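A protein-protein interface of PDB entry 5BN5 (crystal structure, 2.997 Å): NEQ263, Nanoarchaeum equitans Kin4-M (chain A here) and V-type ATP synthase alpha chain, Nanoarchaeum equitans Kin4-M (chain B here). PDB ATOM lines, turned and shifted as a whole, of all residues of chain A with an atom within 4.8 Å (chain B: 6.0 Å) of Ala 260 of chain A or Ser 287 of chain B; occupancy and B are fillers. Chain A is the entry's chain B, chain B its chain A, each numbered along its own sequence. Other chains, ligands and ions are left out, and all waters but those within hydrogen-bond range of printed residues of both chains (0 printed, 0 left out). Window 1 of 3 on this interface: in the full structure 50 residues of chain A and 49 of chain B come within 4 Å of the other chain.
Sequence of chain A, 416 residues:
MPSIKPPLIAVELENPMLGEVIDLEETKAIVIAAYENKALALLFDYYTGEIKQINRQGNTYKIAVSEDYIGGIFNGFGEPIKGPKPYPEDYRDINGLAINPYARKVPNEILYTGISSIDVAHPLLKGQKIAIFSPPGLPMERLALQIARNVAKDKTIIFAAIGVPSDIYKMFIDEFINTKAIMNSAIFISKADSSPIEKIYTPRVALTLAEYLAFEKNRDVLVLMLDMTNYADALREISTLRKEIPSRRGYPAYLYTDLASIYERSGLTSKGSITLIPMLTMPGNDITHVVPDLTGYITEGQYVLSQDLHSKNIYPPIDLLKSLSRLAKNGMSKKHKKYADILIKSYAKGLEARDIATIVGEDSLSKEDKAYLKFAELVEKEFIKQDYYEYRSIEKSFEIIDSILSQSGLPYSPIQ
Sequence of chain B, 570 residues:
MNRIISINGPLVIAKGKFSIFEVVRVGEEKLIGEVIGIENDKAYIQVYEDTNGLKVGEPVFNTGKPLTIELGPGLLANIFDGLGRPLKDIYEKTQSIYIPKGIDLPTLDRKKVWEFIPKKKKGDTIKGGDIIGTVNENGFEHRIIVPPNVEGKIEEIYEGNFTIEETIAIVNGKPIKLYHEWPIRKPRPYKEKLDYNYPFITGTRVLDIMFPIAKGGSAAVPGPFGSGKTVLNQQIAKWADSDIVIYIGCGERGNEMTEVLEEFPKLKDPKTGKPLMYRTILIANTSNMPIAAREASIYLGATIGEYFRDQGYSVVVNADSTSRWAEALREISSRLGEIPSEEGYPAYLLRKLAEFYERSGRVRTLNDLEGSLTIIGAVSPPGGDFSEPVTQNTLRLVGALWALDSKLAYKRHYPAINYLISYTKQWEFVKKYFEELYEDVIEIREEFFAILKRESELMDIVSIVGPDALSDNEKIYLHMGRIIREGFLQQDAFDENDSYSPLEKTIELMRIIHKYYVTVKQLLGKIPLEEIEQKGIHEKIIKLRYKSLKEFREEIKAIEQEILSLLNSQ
N of Gly 254 of chain B sits at hydrogen-bond distance from OE2 of Glu 264 of chain A (3.5 Å). NH2 of Arg 294 of chain B is in hydrogen-bond range of OG1 of Thr 257 of chain A (3.1 Å). O of Ile 298 of chain A sits at hydrogen-bond distance from NE of Arg 253 of chain B (2.8 Å). O of Gly 251 of chain B sits at hydrogen-bond distance from OH of Tyr 256 of chain A, at 3.3 Å.
Of the 12 printed residues of chain B, 7 touch a printed residue of chain A. Printed residues of chain B that touch a printed residue of chain A: Gly 251, Glu 252, Arg 253, Gly 254, Ser 287, Asn 288 and Arg 294. Printed residues of chain A that touch a printed residue of chain B: Tyr 256, Thr 257, Ala 260, Glu 264 and Ile 298.
Ala 260 of chain A touches just these residues of chain B: Ser 287 and Asn 288. Printed residues of chain A within 4 Å of Gly 254 of chain B: Glu 264. Of the printed residues of chain A, Arg 294 of chain B touches Tyr 256 and Thr 257. Printed residues of chain B within 4 Å of Glu 264 of chain A: Glu 252 (3.9997 Å), Arg 253 (3.3 Å), Gly 254 (3.5 Å), Ser 287 (3.4 Å) and Asn 288 (3.5 Å). Of the printed residues of chain A, Arg 253 of chain B touches Glu 264 and Ile 298. Of the printed residues of chain A, Asn 288 of chain B touches Ala 260 (3.5 Å) and Glu 264 (3.5 Å). The nearest residue of chain A that does not touch Ser 287 of chain B is Ile 298 of chain A (4.7 Å). The nearest printed residue of chain A that does not touch Arg 253 of chain B is Tyr 256 of chain A (5.8 Å).
Among the printed residues, pairs that only touch across the chains: Glu 264 of chain A with Arg 253 of chain B (3.3 Å), Ala 260 of chain A with Ser 287 of chain B (3.3 Å), Glu 264 of chain A with Ser 287 of chain B (3.4 Å), Thr 257 of chain A with Ser 287 of chain B (3.5 Å), Ala 260 of chain A with Asn 288 of chain B (3.5 Å), Glu 264 of chain A with Asn 288 of chain B (3.5 Å), Tyr 256 of chain A with Ser 287 of chain B (3.9 Å), Tyr 256 of chain A with Glu 252 of chain B (3.9 Å), Tyr 256 of chain A with Arg 294 of chain B (3.9 Å) and Glu 264 of chain A with Glu 252 of chain B (3.9997 Å).
NH2 of Arg 294 of chain B lies within hydrogen-bond range of O of Ser 287 of chain B (3.3 Å). N of Gly 251 of chain B sits at hydrogen-bond distance from O of Asn 285 of chain B, at 2.8 Å. The side-chain sulfur (SG) of Cys 250 of chain B lies within hydrogen-bond range of the backbone carbonyl oxygen (O) of Arg 294 of chain B (3.7 Å). The backbone carbonyl oxygen of Thr 257 of chain A sits close to the side-chain hydroxyl of Ser 261 of chain A (3.5 Å). ND2 of Asn 285 of chain B lies close to N of Arg 294 of chain B. The backbone carbonyl oxygen of Glu 252 of chain B sits at hydrogen-bond distance from the backbone NH of Ser 287 of chain B, 3.1 Å away.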
ATOM      1  N   TYR A 256      -6.146  26.712 -27.586  1.00  0.00           N
ATOM      2  CA  TYR A 256      -5.285  27.370 -26.610  1.00  0.00           C
ATOM      3  C   TYR A 256      -5.533  26.841 -25.202  1.00  0.00           C
ATOM      4  O   TYR A 256      -4.597  26.449 -24.506  1.00  0.00           O
ATOM      5  CB  TYR A 256      -5.494  28.887 -26.644  1.00  0.00           C
ATOM      6  CG  TYR A 256      -4.650  29.650 -25.645  1.00  0.00           C
ATOM      7  CD1 TYR A 256      -3.358  30.048 -25.960  1.00  0.00           C
ATOM      8  CD2 TYR A 256      -5.148  29.976 -24.389  1.00  0.00           C
ATOM      9  CE1 TYR A 256      -2.584  30.746 -25.053  1.00  0.00           C
ATOM     10  CE2 TYR A 256      -4.380  30.671 -23.474  1.00  0.00           C
ATOM     11  CZ  TYR A 256      -3.099  31.054 -23.811  1.00  0.00           C
ATOM     12  OH  TYR A 256      -2.332  31.749 -22.905  1.00  0.00           O
ATOM     13  N   THR A 257      -6.798  26.833 -24.793  1.00  0.00           N
ATOM     14  CA  THR A 257      -7.177  26.394 -23.455  1.00  0.00           C
ATOM     15  C   THR A 257      -6.843  24.920 -23.235  1.00  0.00           C
ATOM     16  O   THR A 257      -6.414  24.525 -22.150  1.00  0.00           O
ATOM     17  CB  THR A 257      -8.679  26.625 -23.194  1.00  0.00           C
ATOM     18  OG1 THR A 257      -9.013  27.989 -23.483  1.00  0.00           O
ATOM     19  CG2 THR A 257      -9.028  26.318 -21.744  1.00  0.00           C
ATOM     20  N   ASP A 258      -7.036  24.112 -24.274  1.00  0.00           N
ATOM     21  CA  ASP A 258      -6.758  22.683 -24.191  1.00  0.00           C
ATOM     22  C   ASP A 258      -5.263  22.422 -24.029  1.00  0.00           C
ATOM     23  O   ASP A 258      -4.856  21.544 -23.268  1.00  0.00           O
ATOM     24  CB  ASP A 258      -7.295  21.958 -25.424  1.00  0.00           C
ATOM     25  CG  ASP A 258      -7.320  20.453 -25.250  1.00  0.00           C
ATOM     26  OD1 ASP A 258      -6.285  19.807 -25.509  1.00  0.00           O
ATOM     27  OD2 ASP A 258      -8.376  19.914 -24.857  1.00  0.00           O
ATOM     28  N   LEU A 259      -4.448  23.187 -24.751  1.00  0.00           N
ATOM     29  CA  LEU A 259      -2.999  23.102 -24.612  1.00  0.00           C
ATOM     30  C   LEU A 259      -2.562  23.720 -23.292  1.00  0.00           C
ATOM     31  O   LEU A 259      -1.497  23.397 -22.764  1.00  0.00           O
ATOM     32  CB  LEU A 259      -2.299  23.806 -25.775  1.00  0.00           C
ATOM     33  CG  LEU A 259      -2.427  23.151 -27.152  1.00  0.00           C
ATOM     34  CD1 LEU A 259      -1.666  23.953 -28.196  1.00  0.00           C
ATOM     35  CD2 LEU A 259      -1.934  21.715 -27.108  1.00  0.00           C
ATOM     36  N   ALA A 260      -3.393  24.613 -22.766  1.00  0.00           N
ATOM     37  CA  ALA A 260      -3.124  25.254 -21.487  1.00  0.00           C
ATOM     38  C   ALA A 260      -3.551  24.354 -20.337  1.00  0.00           C
ATOM     39  O   ALA A 260      -3.120  24.535 -19.200  1.00  0.00           O
ATOM     40  CB  ALA A 260      -3.838  26.586 -21.405  1.00  0.00           C
ATOM     41  N   SER A 261      -4.402  23.378 -20.640  1.00  0.00           N
ATOM     42  CA  SER A 261      -4.855  22.420 -19.638  1.00  0.00           C
ATOM     43  C   SER A 261      -3.844  21.289 -19.482  1.00  0.00           C
ATOM     44  O   SER A 261      -4.137  20.257 -18.878  1.00  0.00           O
ATOM     45  CB  SER A 261      -6.227  21.857 -20.014  1.00  0.00           C
ATOM     46  OG  SER A 261      -6.183  21.196 -21.267  1.00  0.00           O
ATOM     47  N   ILE A 262      -2.654  21.494 -20.037  1.00  0.00           N
ATOM     48  CA  ILE A 262      -1.575  20.520 -19.954  1.00  0.00           C
ATOM     49  C   ILE A 262      -0.307  21.176 -19.424  1.00  0.00           C
ATOM     50  O   ILE A 262       0.298  20.699 -18.464  1.00  0.00           O
ATOM     51  CB  ILE A 262      -1.276  19.898 -21.330  1.00  0.00           C
ATOM     52  CG1 ILE A 262      -2.456  19.047 -21.796  1.00  0.00           C
ATOM     53  CG2 ILE A 262      -0.004  19.064 -21.279  1.00  0.00           C
ATOM     54  CD1 ILE A 262      -2.197  18.323 -23.089  1.00  0.00           C
ATOM     55  N   TYR A 263       0.086  22.279 -20.053  1.00  0.00           N
ATOM     56  CA  TYR A 263       1.306  22.984 -19.676  1.00  0.00           C
ATOM     57  C   TYR A 263       1.193  23.567 -18.269  1.00  0.00           C
ATOM     58  O   TYR A 263       2.166  23.589 -17.516  1.00  0.00           O
ATOM     59  CB  TYR A 263       1.624  24.092 -20.684  1.00  0.00           C
ATOM     60  CG  TYR A 263       1.787  23.614 -22.113  1.00  0.00           C
ATOM     61  CD1 TYR A 263       2.127  22.297 -22.397  1.00  0.00           C
ATOM     62  CD2 TYR A 263       1.600  24.484 -23.181  1.00  0.00           C
ATOM     63  CE1 TYR A 263       2.274  21.861 -23.702  1.00  0.00           C
ATOM     64  CE2 TYR A 263       1.746  24.059 -24.487  1.00  0.00           C
ATOM     65  CZ  TYR A 263       2.084  22.747 -24.743  1.00  0.00           C
ATOM     66  OH  TYR A 263       2.231  22.320 -26.042  1.00  0.00           O
ATOM     67  N   GLU A 264      -0.004  24.030 -17.917  1.00  0.00           N
ATOM     68  CA  GLU A 264      -0.250  24.598 -16.595  1.00  0.00           C
ATOM     69  C   GLU A 264      -0.266  23.535 -15.503  1.00  0.00           C
ATOM     70  O   GLU A 264      -0.203  23.853 -14.315  1.00  0.00           O
ATOM     71  CB  GLU A 264      -1.560  25.389 -16.578  1.00  0.00           C
ATOM     72  CG  GLU A 264      -1.465  26.751 -17.236  1.00  0.00           C
ATOM     73  CD  GLU A 264      -0.576  27.704 -16.465  1.00  0.00           C
ATOM     74  OE1 GLU A 264       0.086  28.550 -17.102  1.00  0.00           O
ATOM     75  OE2 GLU A 264      -0.540  27.608 -15.219  1.00  0.00           O
ATOM     76  N   ILE A 298       1.931  29.961 -23.996  1.00  0.00           N
ATOM     77  CA  ILE A 298       1.690  29.276 -22.731  1.00  0.00           C
ATOM     78  C   ILE A 298       2.993  28.886 -22.037  1.00  0.00           C
ATOM     79  O   ILE A 298       3.196  29.199 -20.864  1.00  0.00           O
ATOM     80  CB  ILE A 298       0.831  28.013 -22.924  1.00  0.00           C
ATOM     81  CG1 ILE A 298      -0.422  28.337 -23.736  1.00  0.00           C
ATOM     82  CG2 ILE A 298       0.452  27.419 -21.577  1.00  0.00           C
ATOM     83  CD1 ILE A 298      -1.258  27.126 -24.080  1.00  0.00           C
ATOM     84  N   CYS B 250      -5.889  37.536 -17.100  1.00  0.00           N
ATOM     85  CA  CYS B 250      -6.937  36.872 -17.867  1.00  0.00           C
ATOM     86  C   CYS B 250      -6.387  35.779 -18.778  1.00  0.00           C
ATOM     87  O   CYS B 250      -5.846  36.063 -19.846  1.00  0.00           O
ATOM     88  CB  CYS B 250      -7.724  37.895 -18.692  1.00  0.00           C
ATOM     89  SG  CYS B 250      -9.113  37.199 -19.617  1.00  0.00           S
ATOM     90  N   GLY B 251      -6.529  34.530 -18.344  1.00  0.00           N
ATOM     91  CA  GLY B 251      -6.145  33.384 -19.147  1.00  0.00           C
ATOM     92  C   GLY B 251      -4.665  33.301 -19.467  1.00  0.00           C
ATOM     93  O   GLY B 251      -4.286  32.979 -20.593  1.00  0.00           O
ATOM     94  N   GLU B 252      -3.825  33.588 -18.479  1.00  0.00           N
ATOM     95  CA  GLU B 252      -2.380  33.525 -18.672  1.00  0.00           C
ATOM     96  C   GLU B 252      -1.714  32.557 -17.698  1.00  0.00           C
ATOM     97  O   GLU B 252      -2.375  31.703 -17.105  1.00  0.00           O
ATOM     98  CB  GLU B 252      -1.754  34.917 -18.553  1.00  0.00           C
ATOM     99  CG  GLU B 252      -2.154  35.872 -19.666  1.00  0.00           C
ATOM    100  CD  GLU B 252      -1.686  35.407 -21.032  1.00  0.00           C
ATOM    101  OE1 GLU B 252      -0.642  34.726 -21.108  1.00  0.00           O
ATOM    102  OE2 GLU B 252      -2.366  35.720 -22.033  1.00  0.00           O
ATOM    103  N   ARG B 253      -0.402  32.696 -17.542  1.00  0.00           N
ATOM    104  CA  ARG B 253       0.371  31.805 -16.684  1.00  0.00           C
ATOM    105  C   ARG B 253       0.085  32.053 -15.206  1.00  0.00           C
ATOM    106  O   ARG B 253       0.017  33.198 -14.759  1.00  0.00           O
ATOM    107  CB  ARG B 253       1.868  31.961 -16.966  1.00  0.00           C
ATOM    108  CG  ARG B 253       2.253  31.696 -18.413  1.00  0.00           C
ATOM    109  CD  ARG B 253       3.731  31.957 -18.659  1.00  0.00           C
ATOM    110  NE  ARG B 253       4.094  31.725 -20.053  1.00  0.00           N
ATOM    111  CZ  ARG B 253       4.020  32.647 -21.009  1.00  0.00           C
ATOM    112  NH1 ARG B 253       3.595  33.870 -20.721  1.00  0.00           N
ATOM    113  NH2 ARG B 253       4.369  32.347 -22.252  1.00  0.00           N
ATOM    114  N   GLY B 254      -0.082  30.970 -14.453  1.00  0.00           N
ATOM    115  CA  GLY B 254      -0.338  31.059 -13.028  1.00  0.00           C
ATOM    116  C   GLY B 254       0.871  31.557 -12.262  1.00  0.00           C
ATOM    117  O   GLY B 254       0.740  32.161 -11.197  1.00  0.00           O
ATOM    118  N   ASN B 285      -7.805  34.482 -13.118  1.00  0.00           N
ATOM    119  CA  ASN B 285      -8.465  33.391 -13.820  1.00  0.00           C
ATOM    120  C   ASN B 285      -7.564  32.896 -14.944  1.00  0.00           C
ATOM    121  O   ASN B 285      -7.686  33.328 -16.091  1.00  0.00           O
ATOM    122  CB  ASN B 285      -9.824  33.825 -14.365  1.00  0.00           C
ATOM    123  CG  ASN B 285     -10.611  32.669 -14.945  1.00  0.00           C
ATOM    124  OD1 ASN B 285     -11.083  31.796 -14.214  1.00  0.00           O
ATOM    125  ND2 ASN B 285     -10.759  32.653 -16.264  1.00  0.00           N
ATOM    126  N   THR B 286      -6.654  31.989 -14.600  1.00  0.00           N
ATOM    127  CA  THR B 286      -5.601  31.555 -15.511  1.00  0.00           C
ATOM    128  C   THR B 286      -6.117  30.793 -16.729  1.00  0.00           C
ATOM    129  O   THR B 286      -7.319  30.574 -16.883  1.00  0.00           O
ATOM    130  CB  THR B 286      -4.544  30.696 -14.788  1.00  0.00           C
ATOM    131  OG1 THR B 286      -5.119  29.440 -14.408  1.00  0.00           O
ATOM    132  CG2 THR B 286      -4.030  31.414 -13.548  1.00  0.00           C
ATOM    133  N   SER B 287      -5.187  30.387 -17.587  1.00  0.00           N
ATOM    134  CA  SER B 287      -5.521  29.753 -18.855  1.00  0.00           C
ATOM    135  C   SER B 287      -6.148  28.370 -18.690  1.00  0.00           C
ATOM    136  O   SER B 287      -6.965  27.951 -19.510  1.00  0.00           O
ATOM    137  CB  SER B 287      -4.279  29.670 -19.743  1.00  0.00           C
ATOM    138  OG  SER B 287      -3.244  28.944 -19.102  1.00  0.00           O
ATOM    139  N   ASN B 288      -5.764  27.661 -17.633  1.00  0.00           N
ATOM    140  CA  ASN B 288      -6.313  26.334 -17.370  1.00  0.00           C
ATOM    141  C   ASN B 288      -7.614  26.397 -16.575  1.00  0.00           C
ATOM    142  O   ASN B 288      -8.368  25.425 -16.514  1.00  0.00           O
ATOM    143  CB  ASN B 288      -5.287  25.450 -16.656  1.00  0.00           C
ATOM    144  CG  ASN B 288      -4.814  26.048 -15.347  1.00  0.00           C
ATOM    145  OD1 ASN B 288      -4.800  27.267 -15.176  1.00  0.00           O
ATOM    146  ND2 ASN B 288      -4.419  25.190 -14.413  1.00  0.00           N
ATOM    147  N   MET B 289      -7.868  27.550 -15.964  1.00  0.00           N
ATOM    148  CA  MET B 289      -9.110  27.789 -15.242  1.00  0.00           C
ATOM    149  C   MET B 289     -10.259  27.960 -16.238  1.00  0.00           C
ATOM    150  O   MET B 289     -10.011  28.246 -17.410  1.00  0.00           O
ATOM    151  CB  MET B 289      -8.963  29.027 -14.350  1.00  0.00           C
ATOM    152  CG  MET B 289      -7.992  28.831 -13.196  1.00  0.00           C
ATOM    153  SD  MET B 289      -7.843  30.278 -12.129  1.00  0.00           S
ATOM    154  CE  MET B 289      -9.509  30.400 -11.488  1.00  0.00           C
ATOM    155  N   PRO B 290     -11.513  27.759 -15.783  1.00  0.00           N
ATOM    156  CA  PRO B 290     -12.712  27.893 -16.621  1.00  0.00           C
ATOM    157  C   PRO B 290     -12.690  29.107 -17.549  1.00  0.00           C
ATOM    158  O   PRO B 290     -12.407  30.223 -17.115  1.00  0.00           O
ATOM    159  CB  PRO B 290     -13.827  28.035 -15.589  1.00  0.00           C
ATOM    160  CG  PRO B 290     -13.370  27.178 -14.466  1.00  0.00           C
ATOM    161  CD  PRO B 290     -11.861  27.287 -14.428  1.00  0.00           C
ATOM    162  N   ARG B 294     -13.218  34.070 -17.674  1.00  0.00           N
ATOM    163  CA  ARG B 294     -12.337  35.055 -18.288  1.00  0.00           C
ATOM    164  C   ARG B 294     -13.098  36.353 -18.524  1.00  0.00           C
ATOM    165  O   ARG B 294     -12.580  37.444 -18.288  1.00  0.00           O
ATOM    166  CB  ARG B 294     -11.786  34.539 -19.617  1.00  0.00           C
ATOM    167  CG  ARG B 294     -10.850  33.350 -19.500  1.00  0.00           C
ATOM    168  CD  ARG B 294     -10.326  32.944 -20.867  1.00  0.00           C
ATOM    169  NE  ARG B 294      -9.381  31.833 -20.793  1.00  0.00           N
ATOM    170  CZ  ARG B 294      -8.794  31.282 -21.850  1.00  0.00           C
ATOM    171  NH1 ARG B 294      -9.054  31.738 -23.068  1.00  0.00           N
ATOM    172  NH2 ARG B 294      -7.946  30.275 -21.690  1.00  0.00           N
